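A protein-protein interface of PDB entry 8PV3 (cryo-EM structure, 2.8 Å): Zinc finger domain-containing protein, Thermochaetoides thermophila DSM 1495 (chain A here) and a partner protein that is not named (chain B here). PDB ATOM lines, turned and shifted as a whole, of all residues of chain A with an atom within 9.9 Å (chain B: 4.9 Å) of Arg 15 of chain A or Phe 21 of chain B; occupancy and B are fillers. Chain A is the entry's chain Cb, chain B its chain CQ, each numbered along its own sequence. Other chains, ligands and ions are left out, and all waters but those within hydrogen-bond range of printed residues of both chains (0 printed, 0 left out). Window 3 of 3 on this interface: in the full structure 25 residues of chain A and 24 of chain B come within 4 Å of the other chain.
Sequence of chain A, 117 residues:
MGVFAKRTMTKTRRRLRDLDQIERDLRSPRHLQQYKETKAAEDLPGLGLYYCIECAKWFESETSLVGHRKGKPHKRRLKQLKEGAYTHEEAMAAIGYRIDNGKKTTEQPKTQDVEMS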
ATOM      1  N   THR A   8      -0.292  -1.395  29.320  1.00  0.00           N
ATOM      2  CA  THR A   8       0.525  -1.996  28.275  1.00  0.00           C
ATOM      3  C   THR A   8      -0.287  -2.354  27.038  1.00  0.00           C
ATOM      4  O   THR A   8       0.080  -3.282  26.309  1.00  0.00           O
ATOM      5  CB  THR A   8       1.244  -3.233  28.811  1.00  0.00           C
ATOM      6  OG1 THR A   8       0.324  -4.038  29.558  1.00  0.00           O
ATOM      7  CG2 THR A   8       2.398  -2.825  29.707  1.00  0.00           C
ATOM      8  N   MET A   9      -1.385  -1.636  26.791  1.00  0.00           N
ATOM      9  CA  MET A   9      -2.264  -1.942  25.670  1.00  0.00           C
ATOM     10  C   MET A   9      -1.604  -1.671  24.324  1.00  0.00           C
ATOM     11  O   MET A   9      -1.868  -2.397  23.359  1.00  0.00           O
ATOM     12  CB  MET A   9      -3.558  -1.134  25.809  1.00  0.00           C
ATOM     13  CG  MET A   9      -4.602  -1.388  24.738  1.00  0.00           C
ATOM     14  SD  MET A   9      -6.097  -0.416  24.998  1.00  0.00           S
ATOM     15  CE  MET A   9      -5.514   1.224  24.579  1.00  0.00           C
ATOM     16  N   THR A  10      -0.735  -0.668  24.242  1.00  0.00           N
ATOM     17  CA  THR A  10      -0.131  -0.261  22.981  1.00  0.00           C
ATOM     18  C   THR A  10       1.170  -0.989  22.669  1.00  0.00           C
ATOM     19  O   THR A  10       1.824  -0.648  21.680  1.00  0.00           O
ATOM     20  CB  THR A  10       0.121   1.247  22.977  1.00  0.00           C
ATOM     21  OG1 THR A  10       0.823   1.615  24.171  1.00  0.00           O
ATOM     22  CG2 THR A  10      -1.194   2.002  22.914  1.00  0.00           C
ATOM     23  N   LYS A  11       1.564  -1.967  23.482  1.00  0.00           N
ATOM     24  CA  LYS A  11       2.775  -2.727  23.205  1.00  0.00           C
ATOM     25  C   LYS A  11       2.594  -3.593  21.964  1.00  0.00           C
ATOM     26  O   LYS A  11       1.474  -3.918  21.563  1.00  0.00           O
ATOM     27  CB  LYS A  11       3.144  -3.603  24.402  1.00  0.00           C
ATOM     28  CG  LYS A  11       3.953  -2.893  25.471  1.00  0.00           C
ATOM     29  CD  LYS A  11       4.278  -3.830  26.616  1.00  0.00           C
ATOM     30  CE  LYS A  11       5.366  -3.264  27.505  1.00  0.00           C
ATOM     31  NZ  LYS A  11       6.702  -3.381  26.883  1.00  0.00           N
ATOM     32  N   THR A  12       3.722  -3.956  21.347  1.00  0.00           N
ATOM     33  CA  THR A  12       3.678  -4.777  20.142  1.00  0.00           C
ATOM     34  C   THR A  12       3.188  -6.189  20.442  1.00  0.00           C
ATOM     35  O   THR A  12       2.480  -6.787  19.623  1.00  0.00           O
ATOM     36  CB  THR A  12       5.062  -4.811  19.486  1.00  0.00           C
ATOM     37  OG1 THR A  12       5.558  -3.474  19.347  1.00  0.00           O
ATOM     38  CG2 THR A  12       4.992  -5.442  18.107  1.00  0.00           C
ATOM     39  N   ARG A  13       3.524  -6.730  21.614  1.00  0.00           N
ATOM     40  CA  ARG A  13       3.059  -8.063  21.985  1.00  0.00           C
ATOM     41  C   ARG A  13       1.577  -8.105  22.345  1.00  0.00           C
ATOM     42  O   ARG A  13       1.034  -9.202  22.511  1.00  0.00           O
ATOM     43  CB  ARG A  13       3.892  -8.609  23.147  1.00  0.00           C
ATOM     44  CG  ARG A  13       3.774  -7.834  24.446  1.00  0.00           C
ATOM     45  CD  ARG A  13       4.354  -8.635  25.601  1.00  0.00           C
ATOM     46  NE  ARG A  13       4.698  -7.797  26.744  1.00  0.00           N
ATOM     47  CZ  ARG A  13       3.864  -7.481  27.723  1.00  0.00           C
ATOM     48  NH1 ARG A  13       2.615  -7.919  27.735  1.00  0.00           N
ATOM     49  NH2 ARG A  13       4.292  -6.708  28.716  1.00  0.00           N
ATOM     50  N   ARG A  14       0.917  -6.955  22.472  1.00  0.00           N
ATOM     51  CA  ARG A  14      -0.521  -6.886  22.696  1.00  0.00           C
ATOM     52  C   ARG A  14      -1.277  -6.426  21.455  1.00  0.00           C
ATOM     53  O   ARG A  14      -2.409  -5.945  21.573  1.00  0.00           O
ATOM     54  CB  ARG A  14      -0.825  -5.956  23.871  1.00  0.00           C
ATOM     55  CG  ARG A  14      -0.281  -6.445  25.202  1.00  0.00           C
ATOM     56  CD  ARG A  14      -1.325  -7.242  25.958  1.00  0.00           C
ATOM     57  NE  ARG A  14      -2.536  -6.462  26.185  1.00  0.00           N
ATOM     58  CZ  ARG A  14      -2.734  -5.678  27.236  1.00  0.00           C
ATOM     59  NH1 ARG A  14      -1.819  -5.548  28.181  1.00  0.00           N
ATOM     60  NH2 ARG A  14      -3.879  -5.011  27.341  1.00  0.00           N
ATOM     61  N   ARG A  15      -0.677  -6.559  20.274  1.00  0.00           N
ATOM     62  CA  ARG A  15      -1.292  -6.081  19.044  1.00  0.00           C
ATOM     63  C   ARG A  15      -2.449  -6.984  18.626  1.00  0.00           C
ATOM     64  O   ARG A  15      -2.454  -8.190  18.891  1.00  0.00           O
ATOM     65  CB  ARG A  15      -0.245  -6.014  17.930  1.00  0.00           C
ATOM     66  CG  ARG A  15      -0.628  -5.144  16.747  1.00  0.00           C
ATOM     67  CD  ARG A  15       0.126  -5.553  15.499  1.00  0.00           C
ATOM     68  NE  ARG A  15      -0.294  -4.774  14.341  1.00  0.00           N
ATOM     69  CZ  ARG A  15      -1.157  -5.198  13.430  1.00  0.00           C
ATOM     70  NH1 ARG A  15      -1.705  -6.399  13.501  1.00  0.00           N
ATOM     71  NH2 ARG A  15      -1.482  -4.395  12.421  1.00  0.00           N
ATOM     72  N   LEU A  16      -3.438  -6.386  17.965  1.00  0.00           N
ATOM     73  CA  LEU A  16      -4.595  -7.099  17.450  1.00  0.00           C
ATOM     74  C   LEU A  16      -4.619  -7.020  15.927  1.00  0.00           C
ATOM     75  O   LEU A  16      -3.848  -6.281  15.310  1.00  0.00           O
ATOM     76  CB  LEU A  16      -5.898  -6.533  18.029  1.00  0.00           C
ATOM     77  CG  LEU A  16      -5.976  -6.445  19.555  1.00  0.00           C
ATOM     78  CD1 LEU A  16      -7.318  -5.889  19.993  1.00  0.00           C
ATOM     79  CD2 LEU A  16      -5.723  -7.803  20.186  1.00  0.00           C
ATOM     80  N   ARG A  17      -5.516  -7.804  15.331  1.00  0.00           N
ATOM     81  CA  ARG A  17      -5.607  -7.888  13.878  1.00  0.00           C
ATOM     82  C   ARG A  17      -6.146  -6.588  13.291  1.00  0.00           C
ATOM     83  O   ARG A  17      -7.006  -5.929  13.880  1.00  0.00           O
ATOM     84  CB  ARG A  17      -6.499  -9.064  13.484  1.00  0.00           C
ATOM     85  CG  ARG A  17      -6.437  -9.454  12.020  1.00  0.00           C
ATOM     86  CD  ARG A  17      -6.917 -10.881  11.828  1.00  0.00           C
ATOM     87  NE  ARG A  17      -6.861 -11.305  10.436  1.00  0.00           N
ATOM     88  CZ  ARG A  17      -5.768 -11.744   9.828  1.00  0.00           C
ATOM     89  NH1 ARG A  17      -4.607 -11.814  10.459  1.00  0.00           N
ATOM     90  NH2 ARG A  17      -5.842 -12.124   8.557  1.00  0.00           N
ATOM     91  N   ASP A  18      -5.635  -6.222  12.118  1.00  0.00           N
ATOM     92  CA  ASP A  18      -5.934  -4.926  11.530  1.00  0.00           C
ATOM     93  C   ASP A  18      -7.199  -5.009  10.677  1.00  0.00           C
ATOM     94  O   ASP A  18      -7.593  -6.079  10.200  1.00  0.00           O
ATOM     95  CB  ASP A  18      -4.742  -4.441  10.696  1.00  0.00           C
ATOM     96  CG  ASP A  18      -4.832  -2.965  10.314  1.00  0.00           C
ATOM     97  OD1 ASP A  18      -5.883  -2.325  10.535  1.00  0.00           O
ATOM     98  OD2 ASP A  18      -3.831  -2.438   9.785  1.00  0.00           O
ATOM     99  N   LEU A  19      -7.828  -3.848  10.480  1.00  0.00           N
ATOM    100  CA  LEU A  19      -9.145  -3.803   9.855  1.00  0.00           C
ATOM    101  C   LEU A  19      -9.065  -4.099   8.359  1.00  0.00           C
ATOM    102  O   LEU A  19      -9.989  -4.688   7.787  1.00  0.00           O
ATOM    103  CB  LEU A  19      -9.785  -2.440  10.114  1.00  0.00           C
ATOM    104  CG  LEU A  19     -11.204  -2.209   9.606  1.00  0.00           C
ATOM    105  CD1 LEU A  19     -12.140  -3.172  10.302  1.00  0.00           C
ATOM    106  CD2 LEU A  19     -11.634  -0.774   9.842  1.00  0.00           C
ATOM    107  N   ASP A  20      -7.967  -3.711   7.704  1.00  0.00           N
ATOM    108  CA  ASP A  20      -7.802  -4.069   6.297  1.00  0.00           C
ATOM    109  C   ASP A  20      -7.541  -5.564   6.140  1.00  0.00           C
ATOM    110  O   ASP A  20      -7.962  -6.176   5.148  1.00  0.00           O
ATOM    111  CB  ASP A  20      -6.683  -3.240   5.662  1.00  0.00           C
ATOM    112  CG  ASP A  20      -5.311  -3.600   6.191  1.00  0.00           C
ATOM    113  OD1 ASP A  20      -5.193  -3.888   7.397  1.00  0.00           O
ATOM    114  OD2 ASP A  20      -4.346  -3.596   5.397  1.00  0.00           O
ATOM    115  N   GLN A  21      -6.867  -6.173   7.121  1.00  0.00           N
ATOM    116  CA  GLN A  21      -6.758  -7.627   7.149  1.00  0.00           C
ATOM    117  C   GLN A  21      -8.124  -8.271   7.321  1.00  0.00           C
ATOM    118  O   GLN A  21      -8.400  -9.315   6.724  1.00  0.00           O
ATOM    119  CB  GLN A  21      -5.814  -8.075   8.263  1.00  0.00           C
ATOM    120  CG  GLN A  21      -4.391  -7.576   8.127  1.00  0.00           C
ATOM    121  CD  GLN A  21      -3.510  -8.022   9.275  1.00  0.00           C
ATOM    122  OE1 GLN A  21      -3.633  -7.531  10.395  1.00  0.00           O
ATOM    123  NE2 GLN A  21      -2.617  -8.965   9.001  1.00  0.00           N
ATOM    124  N   ILE A  22      -8.994  -7.655   8.128  1.00  0.00           N
ATOM    125  CA  ILE A  22     -10.359  -8.158   8.282  1.00  0.00           C
ATOM    126  C   ILE A  22     -11.128  -8.041   6.968  1.00  0.00           C
ATOM    127  O   ILE A  22     -11.899  -8.938   6.600  1.00  0.00           O
ATOM    128  CB  ILE A  22     -11.065  -7.419   9.433  1.00  0.00           C
ATOM    129  CG1 ILE A  22     -10.354  -7.730  10.745  1.00  0.00           C
ATOM    130  CG2 ILE A  22     -12.528  -7.817   9.537  1.00  0.00           C
ATOM    131  CD1 ILE A  22     -10.259  -9.198  11.015  1.00  0.00           C
ATOM    132  N   HIS A  31      -6.938 -15.982   2.864  1.00  0.00           N
ATOM    133  CA  HIS A  31      -6.214 -15.224   3.881  1.00  0.00           C
ATOM    134  C   HIS A  31      -6.709 -15.595   5.277  1.00  0.00           C
ATOM    135  O   HIS A  31      -5.915 -15.724   6.220  1.00  0.00           O
ATOM    136  CB  HIS A  31      -6.392 -13.725   3.599  1.00  0.00           C
ATOM    137  CG  HIS A  31      -5.622 -12.813   4.508  1.00  0.00           C
ATOM    138  ND1 HIS A  31      -5.721 -11.442   4.422  1.00  0.00           N
ATOM    139  CD2 HIS A  31      -4.696 -13.061   5.465  1.00  0.00           C
ATOM    140  CE1 HIS A  31      -4.926 -10.886   5.318  1.00  0.00           C
ATOM    141  NE2 HIS A  31      -4.290 -11.846   5.963  1.00  0.00           N
ATOM    142  N   TYR A  35      -4.590 -17.216   8.409  1.00  0.00           N
ATOM    143  CA  TYR A  35      -4.644 -16.767   9.797  1.00  0.00           C
ATOM    144  C   TYR A  35      -5.074 -17.903  10.722  1.00  0.00           C
ATOM    145  O   TYR A  35      -4.735 -17.913  11.912  1.00  0.00           O
ATOM    146  CB  TYR A  35      -5.585 -15.569   9.927  1.00  0.00           C
ATOM    147  CG  TYR A  35      -5.744 -15.063  11.342  1.00  0.00           C
ATOM    148  CD1 TYR A  35      -4.641 -14.655  12.082  1.00  0.00           C
ATOM    149  CD2 TYR A  35      -6.994 -14.999  11.941  1.00  0.00           C
ATOM    150  CE1 TYR A  35      -4.779 -14.191  13.375  1.00  0.00           C
ATOM    151  CE2 TYR A  35      -7.143 -14.538  13.233  1.00  0.00           C
ATOM    152  CZ  TYR A  35      -6.033 -14.136  13.945  1.00  0.00           C
ATOM    153  OH  TYR A  35      -6.179 -13.676  15.233  1.00  0.00           O
ATOM    154  N   LYS A  39      -2.457 -20.173  14.039  1.00  0.00           N
ATOM    155  CA  LYS A  39      -2.814 -20.450  15.421  1.00  0.00           C
ATOM    156  C   LYS A  39      -2.964 -21.953  15.622  1.00  0.00           C
ATOM    157  O   LYS A  39      -3.087 -22.722  14.666  1.00  0.00           O
ATOM    158  CB  LYS A  39      -4.112 -19.737  15.821  1.00  0.00           C
ATOM    159  CG  LYS A  39      -4.046 -18.220  15.735  1.00  0.00           C
ATOM    160  CD  LYS A  39      -2.996 -17.656  16.679  1.00  0.00           C
ATOM    161  CE  LYS A  39      -3.381 -17.873  18.134  1.00  0.00           C
ATOM    162  NZ  LYS A  39      -4.613 -17.125  18.509  1.00  0.00           N
ATOM    163  N   ALA A  56     -12.778 -10.461  14.769  1.00  0.00           N
ATOM    164  CA  ALA A  56     -11.537 -11.248  14.759  1.00  0.00           C
ATOM    165  C   ALA A  56     -11.312 -11.975  16.081  1.00  0.00           C
ATOM    166  O   ALA A  56     -10.202 -12.017  16.615  1.00  0.00           O
ATOM    167  CB  ALA A  56     -10.326 -10.379  14.416  1.00  0.00           C
ATOM    168  N   ARG A  77     -17.562  -2.526  14.846  1.00  0.00           N
ATOM    169  CA  ARG A  77     -16.813  -3.211  13.796  1.00  0.00           C
ATOM    170  C   ARG A  77     -17.600  -3.258  12.491  1.00  0.00           C
ATOM    171  O   ARG A  77     -17.033  -3.051  11.409  1.00  0.00           O
ATOM    172  CB  ARG A  77     -16.433  -4.620  14.247  1.00  0.00           C
ATOM    173  CG  ARG A  77     -15.073  -4.692  14.907  1.00  0.00           C
ATOM    174  CD  ARG A  77     -13.981  -4.309  13.920  1.00  0.00           C
ATOM    175  NE  ARG A  77     -12.703  -4.077  14.580  1.00  0.00           N
ATOM    176  CZ  ARG A  77     -11.816  -5.026  14.836  1.00  0.00           C
ATOM    177  NH1 ARG A  77     -12.020  -6.279  14.467  1.00  0.00           N
ATOM    178  NH2 ARG A  77     -10.693  -4.710  15.475  1.00  0.00           N
ATOM    179  N   HIS A  88      -3.276   1.264   1.227  1.00  0.00           N
ATOM    180  CA  HIS A  88      -2.237   1.985   0.501  1.00  0.00           C
ATOM    181  C   HIS A  88      -2.784   2.652  -0.754  1.00  0.00           C
ATOM    182  O   HIS A  88      -2.263   3.690  -1.176  1.00  0.00           O
ATOM    183  CB  HIS A  88      -1.095   1.036   0.142  1.00  0.00           C
ATOM    184  CG  HIS A  88      -0.088   0.863   1.235  1.00  0.00           C
ATOM    185  ND1 HIS A  88      -0.185  -0.129   2.186  1.00  0.00           N
ATOM    186  CD2 HIS A  88       1.039   1.553   1.528  1.00  0.00           C
ATOM    187  CE1 HIS A  88       0.837  -0.042   3.017  1.00  0.00           C
ATOM    188  NE2 HIS A  88       1.596   0.970   2.640  1.00  0.00           N
ATOM    189  N   ILE B  19       9.517   6.089  11.194  1.00  0.00           N
ATOM    190  CA  ILE B  19       9.728   4.675  11.484  1.00  0.00           C
ATOM    191  C   ILE B  19       8.870   3.850  10.534  1.00  0.00           C
ATOM    192  O   ILE B  19       7.855   4.321  10.017  1.00  0.00           O
ATOM    193  CB  ILE B  19       9.432   4.363  12.974  1.00  0.00           C
ATOM    194  CG1 ILE B  19      10.099   3.059  13.415  1.00  0.00           C
ATOM    195  CG2 ILE B  19       7.940   4.320  13.244  1.00  0.00           C
ATOM    196  CD1 ILE B  19      10.037   2.814  14.902  1.00  0.00           C
ATOM    197  N   THR B  20       9.294   2.618  10.269  1.00  0.00           N
ATOM    198  CA  THR B  20       8.594   1.772   9.316  1.00  0.00           C
ATOM    199  C   THR B  20       8.151   0.492  10.015  1.00  0.00           C
ATOM    200  O   THR B  20       8.937  -0.129  10.731  1.00  0.00           O
ATOM    201  CB  THR B  20       9.484   1.447   8.119  1.00  0.00           C
ATOM    202  OG1 THR B  20       9.930   2.667   7.533  1.00  0.00           O
ATOM    203  CG2 THR B  20       8.662   0.790   7.054  1.00  0.00           C
ATOM    204  N   PHE B  21       6.900   0.098   9.802  1.00  0.00           N
ATOM    205  CA  PHE B  21       6.328  -1.084  10.429  1.00  0.00           C
ATOM    206  C   PHE B  21       6.252  -2.222   9.417  1.00  0.00           C
ATOM    207  O   PHE B  21       5.664  -2.069   8.341  1.00  0.00           O
ATOM    208  CB  PHE B  21       4.939  -0.781  10.996  1.00  0.00           C
ATOM    209  CG  PHE B  21       4.203  -1.993  11.493  1.00  0.00           C
ATOM    210  CD1 PHE B  21       4.793  -2.855  12.401  1.00  0.00           C
ATOM    211  CD2 PHE B  21       2.912  -2.253  11.075  1.00  0.00           C
ATOM    212  CE1 PHE B  21       4.113  -3.965  12.861  1.00  0.00           C
ATOM    213  CE2 PHE B  21       2.229  -3.355  11.533  1.00  0.00           C
ATOM    214  CZ  PHE B  21       2.828  -4.211  12.428  1.00  0.00           C
ATOM    215  N   MET B  22       6.847  -3.354   9.778  1.00  0.00           N
ATOM    216  CA  MET B  22       6.865  -4.571   8.977  1.00  0.00           C
ATOM    217  C   MET B  22       5.708  -5.441   9.446  1.00  0.00           C
ATOM    218  O   MET B  22       5.712  -5.902  10.592  1.00  0.00           O
ATOM    219  CB  MET B  22       8.175  -5.323   9.200  1.00  0.00           C
ATOM    220  CG  MET B  22       9.499  -4.693   8.752  1.00  0.00           C
ATOM    221  SD  MET B  22       9.741  -4.373   7.007  1.00  0.00           S
ATOM    222  CE  MET B  22       9.454  -2.640   6.906  1.00  0.00           C
ATOM    223  N   ARG B  23       4.717  -5.670   8.588  1.00  0.00           N
ATOM    224  CA  ARG B  23       3.629  -6.558   8.972  1.00  0.00           C
ATOM    225  C   ARG B  23       3.878  -7.967   8.442  1.00  0.00           C
ATOM    226  O   ARG B  23       4.525  -8.163   7.411  1.00  0.00           O
ATOM    227  CB  ARG B  23       2.280  -6.028   8.482  1.00  0.00           C
ATOM    228  CG  ARG B  23       1.120  -6.460   9.365  1.00  0.00           C
ATOM    229  CD  ARG B  23      -0.106  -5.584   9.182  1.00  0.00           C
ATOM    230  NE  ARG B  23      -0.736  -5.759   7.880  1.00  0.00           N
ATOM    231  CZ  ARG B  23      -1.764  -5.043   7.446  1.00  0.00           C
ATOM    232  NH1 ARG B  23      -2.302  -4.090   8.185  1.00  0.00           N
ATOM    233  NH2 ARG B  23      -2.267  -5.294   6.242  1.00  0.00           N
ATOM    234  N   LYS B  27       3.317  -6.376   4.181  1.00  0.00           N
ATOM    235  CA  LYS B  27       3.070  -4.985   3.827  1.00  0.00           C
ATOM    236  C   LYS B  27       3.863  -4.076   4.752  1.00  0.00           C
ATOM    237  O   LYS B  27       3.867  -4.274   5.970  1.00  0.00           O
ATOM    238  CB  LYS B  27       1.580  -4.650   3.921  1.00  0.00           C
ATOM    239  CG  LYS B  27       0.717  -5.335   2.890  1.00  0.00           C
ATOM    240  CD  LYS B  27      -0.722  -4.871   2.990  1.00  0.00           C
ATOM    241  CE  LYS B  27      -1.592  -5.617   1.998  1.00  0.00           C
ATOM    242  NZ  LYS B  27      -1.223  -5.282   0.592  1.00  0.00           N
ATOM    243  N   ALA B  28       4.514  -3.074   4.174  1.00  0.00           N
ATOM    244  CA  ALA B  28       5.344  -2.139   4.918  1.00  0.00           C
ATOM    245  C   ALA B  28       4.638  -0.797   5.048  1.00  0.00           C
ATOM    246  O   ALA B  28       4.088  -0.266   4.080  1.00  0.00           O
ATOM    247  CB  ALA B  28       6.700  -1.949   4.239  1.00  0.00           C
ATOM    248  N   PHE B  29       4.662  -0.249   6.260  1.00  0.00           N
ATOM    249  CA  PHE B  29       3.939   0.977   6.586  1.00  0.00           C
ATOM    250  C   PHE B  29       4.938   2.029   7.040  1.00  0.00           C
ATOM    251  O   PHE B  29       5.497   1.919   8.131  1.00  0.00           O
ATOM    252  CB  PHE B  29       2.895   0.729   7.676  1.00  0.00           C
ATOM    253  CG  PHE B  29       1.849  -0.281   7.306  1.00  0.00           C
ATOM    254  CD1 PHE B  29       2.053  -1.633   7.525  1.00  0.00           C
ATOM    255  CD2 PHE B  29       0.658   0.127   6.742  1.00  0.00           C
ATOM    256  CE1 PHE B  29       1.084  -2.553   7.183  1.00  0.00           C
ATOM    257  CE2 PHE B  29      -0.309  -0.786   6.397  1.00  0.00           C
ATOM    258  CZ  PHE B  29      -0.097  -2.127   6.618  1.00  0.00           C
ATOM    259  N   PHE B  31       5.924   5.707   8.365  1.00  0.00           N
ATOM    260  CA  PHE B  31       5.404   6.851   9.092  1.00  0.00           C
ATOM    261  C   PHE B  31       6.490   7.905   9.219  1.00  0.00           C
ATOM    262  O   PHE B  31       7.643   7.598   9.532  1.00  0.00           O
ATOM    263  CB  PHE B  31       4.911   6.450  10.483  1.00  0.00           C
ATOM    264  CG  PHE B  31       4.006   5.268  10.474  1.00  0.00           C
ATOM    265  CD1 PHE B  31       2.704   5.382  10.023  1.00  0.00           C
ATOM    266  CD2 PHE B  31       4.461   4.034  10.896  1.00  0.00           C
ATOM    267  CE1 PHE B  31       1.876   4.287  10.002  1.00  0.00           C
ATOM    268  CE2 PHE B  31       3.639   2.941  10.877  1.00  0.00           C
ATOM    269  CZ  PHE B  31       2.347   3.066  10.425  1.00  0.00           C
ATOM    270  N   PHE B  40      -1.456   5.184  14.470  1.00  0.00           N
ATOM    271  CA  PHE B  40      -1.633   3.911  13.778  1.00  0.00           C
ATOM    272  C   PHE B  40      -1.684   2.743  14.758  1.00  0.00           C
ATOM    273  O   PHE B  40      -2.485   1.817  14.584  1.00  0.00           O
ATOM    274  CB  PHE B  40      -0.510   3.711  12.763  1.00  0.00           C
ATOM    275  CG  PHE B  40      -0.595   2.417  12.006  1.00  0.00           C
ATOM    276  CD1 PHE B  40      -1.427   2.303  10.907  1.00  0.00           C
ATOM    277  CD2 PHE B  40       0.161   1.317  12.382  1.00  0.00           C
ATOM    278  CE1 PHE B  40      -1.510   1.123  10.207  1.00  0.00           C
ATOM    279  CE2 PHE B  40       0.080   0.136  11.684  1.00  0.00           C
ATOM    280  CZ  PHE B  40      -0.756   0.040  10.595  1.00  0.00           C
ATOM    281  N   LYS B  43      -4.866   2.561  16.323  1.00  0.00           N
ATOM    282  CA  LYS B  43      -5.867   2.133  15.337  1.00  0.00           C
ATOM    283  C   LYS B  43      -6.870   3.243  15.040  1.00  0.00           C
ATOM    284  O   LYS B  43      -8.047   2.984  14.798  1.00  0.00           O
ATOM    285  CB  LYS B  43      -6.597   0.852  15.760  1.00  0.00           C
ATOM    286  CG  LYS B  43      -5.709  -0.296  16.198  1.00  0.00           C
ATOM    287  CD  LYS B  43      -5.079  -1.003  15.018  1.00  0.00           C
ATOM    288  CE  LYS B  43      -4.397  -2.286  15.460  1.00  0.00           C
ATOM    289  NZ  LYS B  43      -3.946  -3.105  14.305  1.00  0.00           N
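The guanidinium group of Arg 23 of chain B lies within salt-bridge range of the side-chain carboxylate of Asp 18 of chain A.
The guanidinium group (NH2) of Arg 23 of chain B lies within salt-bridge range of the side-chain carboxylate (OD2) of Asp 20 of chain A (2.8 Å).
NE2 of His 88 of chain A is in hydrogen-bond range of O of Ala 28 of chain B.
O of Leu 16 of chain A sits at hydrogen-bond distance from NZ of Lys 43 of chain B, 3.3 Å away.
NH2 of Arg 15 of chain A sits close to NZ of Lys 43 of chain B (3.4 Å).
The backbone NH (N) of Phe 21 of chain B is in hydrogen-bond range of the backbone carbonyl oxygen (O) of Phe 29 of chain B (2.8 Å).
The side-chain amide oxygen (OE1) of Gln 21 of chain A lies within hydrogen-bond range of the backbone NH (N) of Asp 18 of chain A (2.9 Å).
Phe 21 of chain B touches Arg 15 of chain A (CZ to NE, 3.7 Å).
Arg 15 of chain A touches Arg 23 of chain B.
NZ of Lys 43 of chain B touches CA of Asp 18 of chain A (3.9 Å).
Gln 21 of chain A touches Arg 23 of chain B.
CE1 of His 88 of chain A touches CE2 of Phe 29 of chain B, at 3.6 Å.
Phe 21 of chain B touches just one residue of chain A: Arg 15 (3.7 Å).
Thr 20 of chain B touches none of the printed residues of chain A.
No residue of chain A comes within 4 Å of Met 22 of chain B.
Printed residues of chain A within 4 Å of Ala 28 of chain B: His 88 (3.1 Å).
Of the printed residues of chain B, Asp 18 of chain A touches Arg 23 and Lys 43.
Of the printed residues of chain B, Leu 16 of chain A touches Lys 43.
Of the printed residues of chain B, Gln 21 of chain A touches Arg 23 (3.6 Å).
Printed residues of chain A within 4 Å of Arg 23 of chain B: Arg 15 (3.7 Å), Asp 18 (2.8 Å), Asp 20 (2.8 Å) and Gln 21 (3.6 Å).
His 31 of chain A touches none of the printed residues of chain B.
Of the 11 printed residues of chain B, 5 touch a printed residue of chain A.
Printed residues of chain B that touch a printed residue of chain A: Phe 21, Arg 23, Ala 28, Phe 29 and Lys 43.
Hydrophobic or aromatic side chains of chain B that line the printed part of chain A: Phe 21 and Phe 29.
Of the 21 printed residues of chain A, 6 touch a printed residue of chain B.
Printed residues of chain A that touch a printed residue of chain B: Arg 15, Leu 16, Asp 18, Asp 20, Gln 21 and His 88.
Along chain A the printed residues that touch a printed residue of chain B span positions 15 to 88.
Among the printed residues, 10 pairs touch across the chains.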
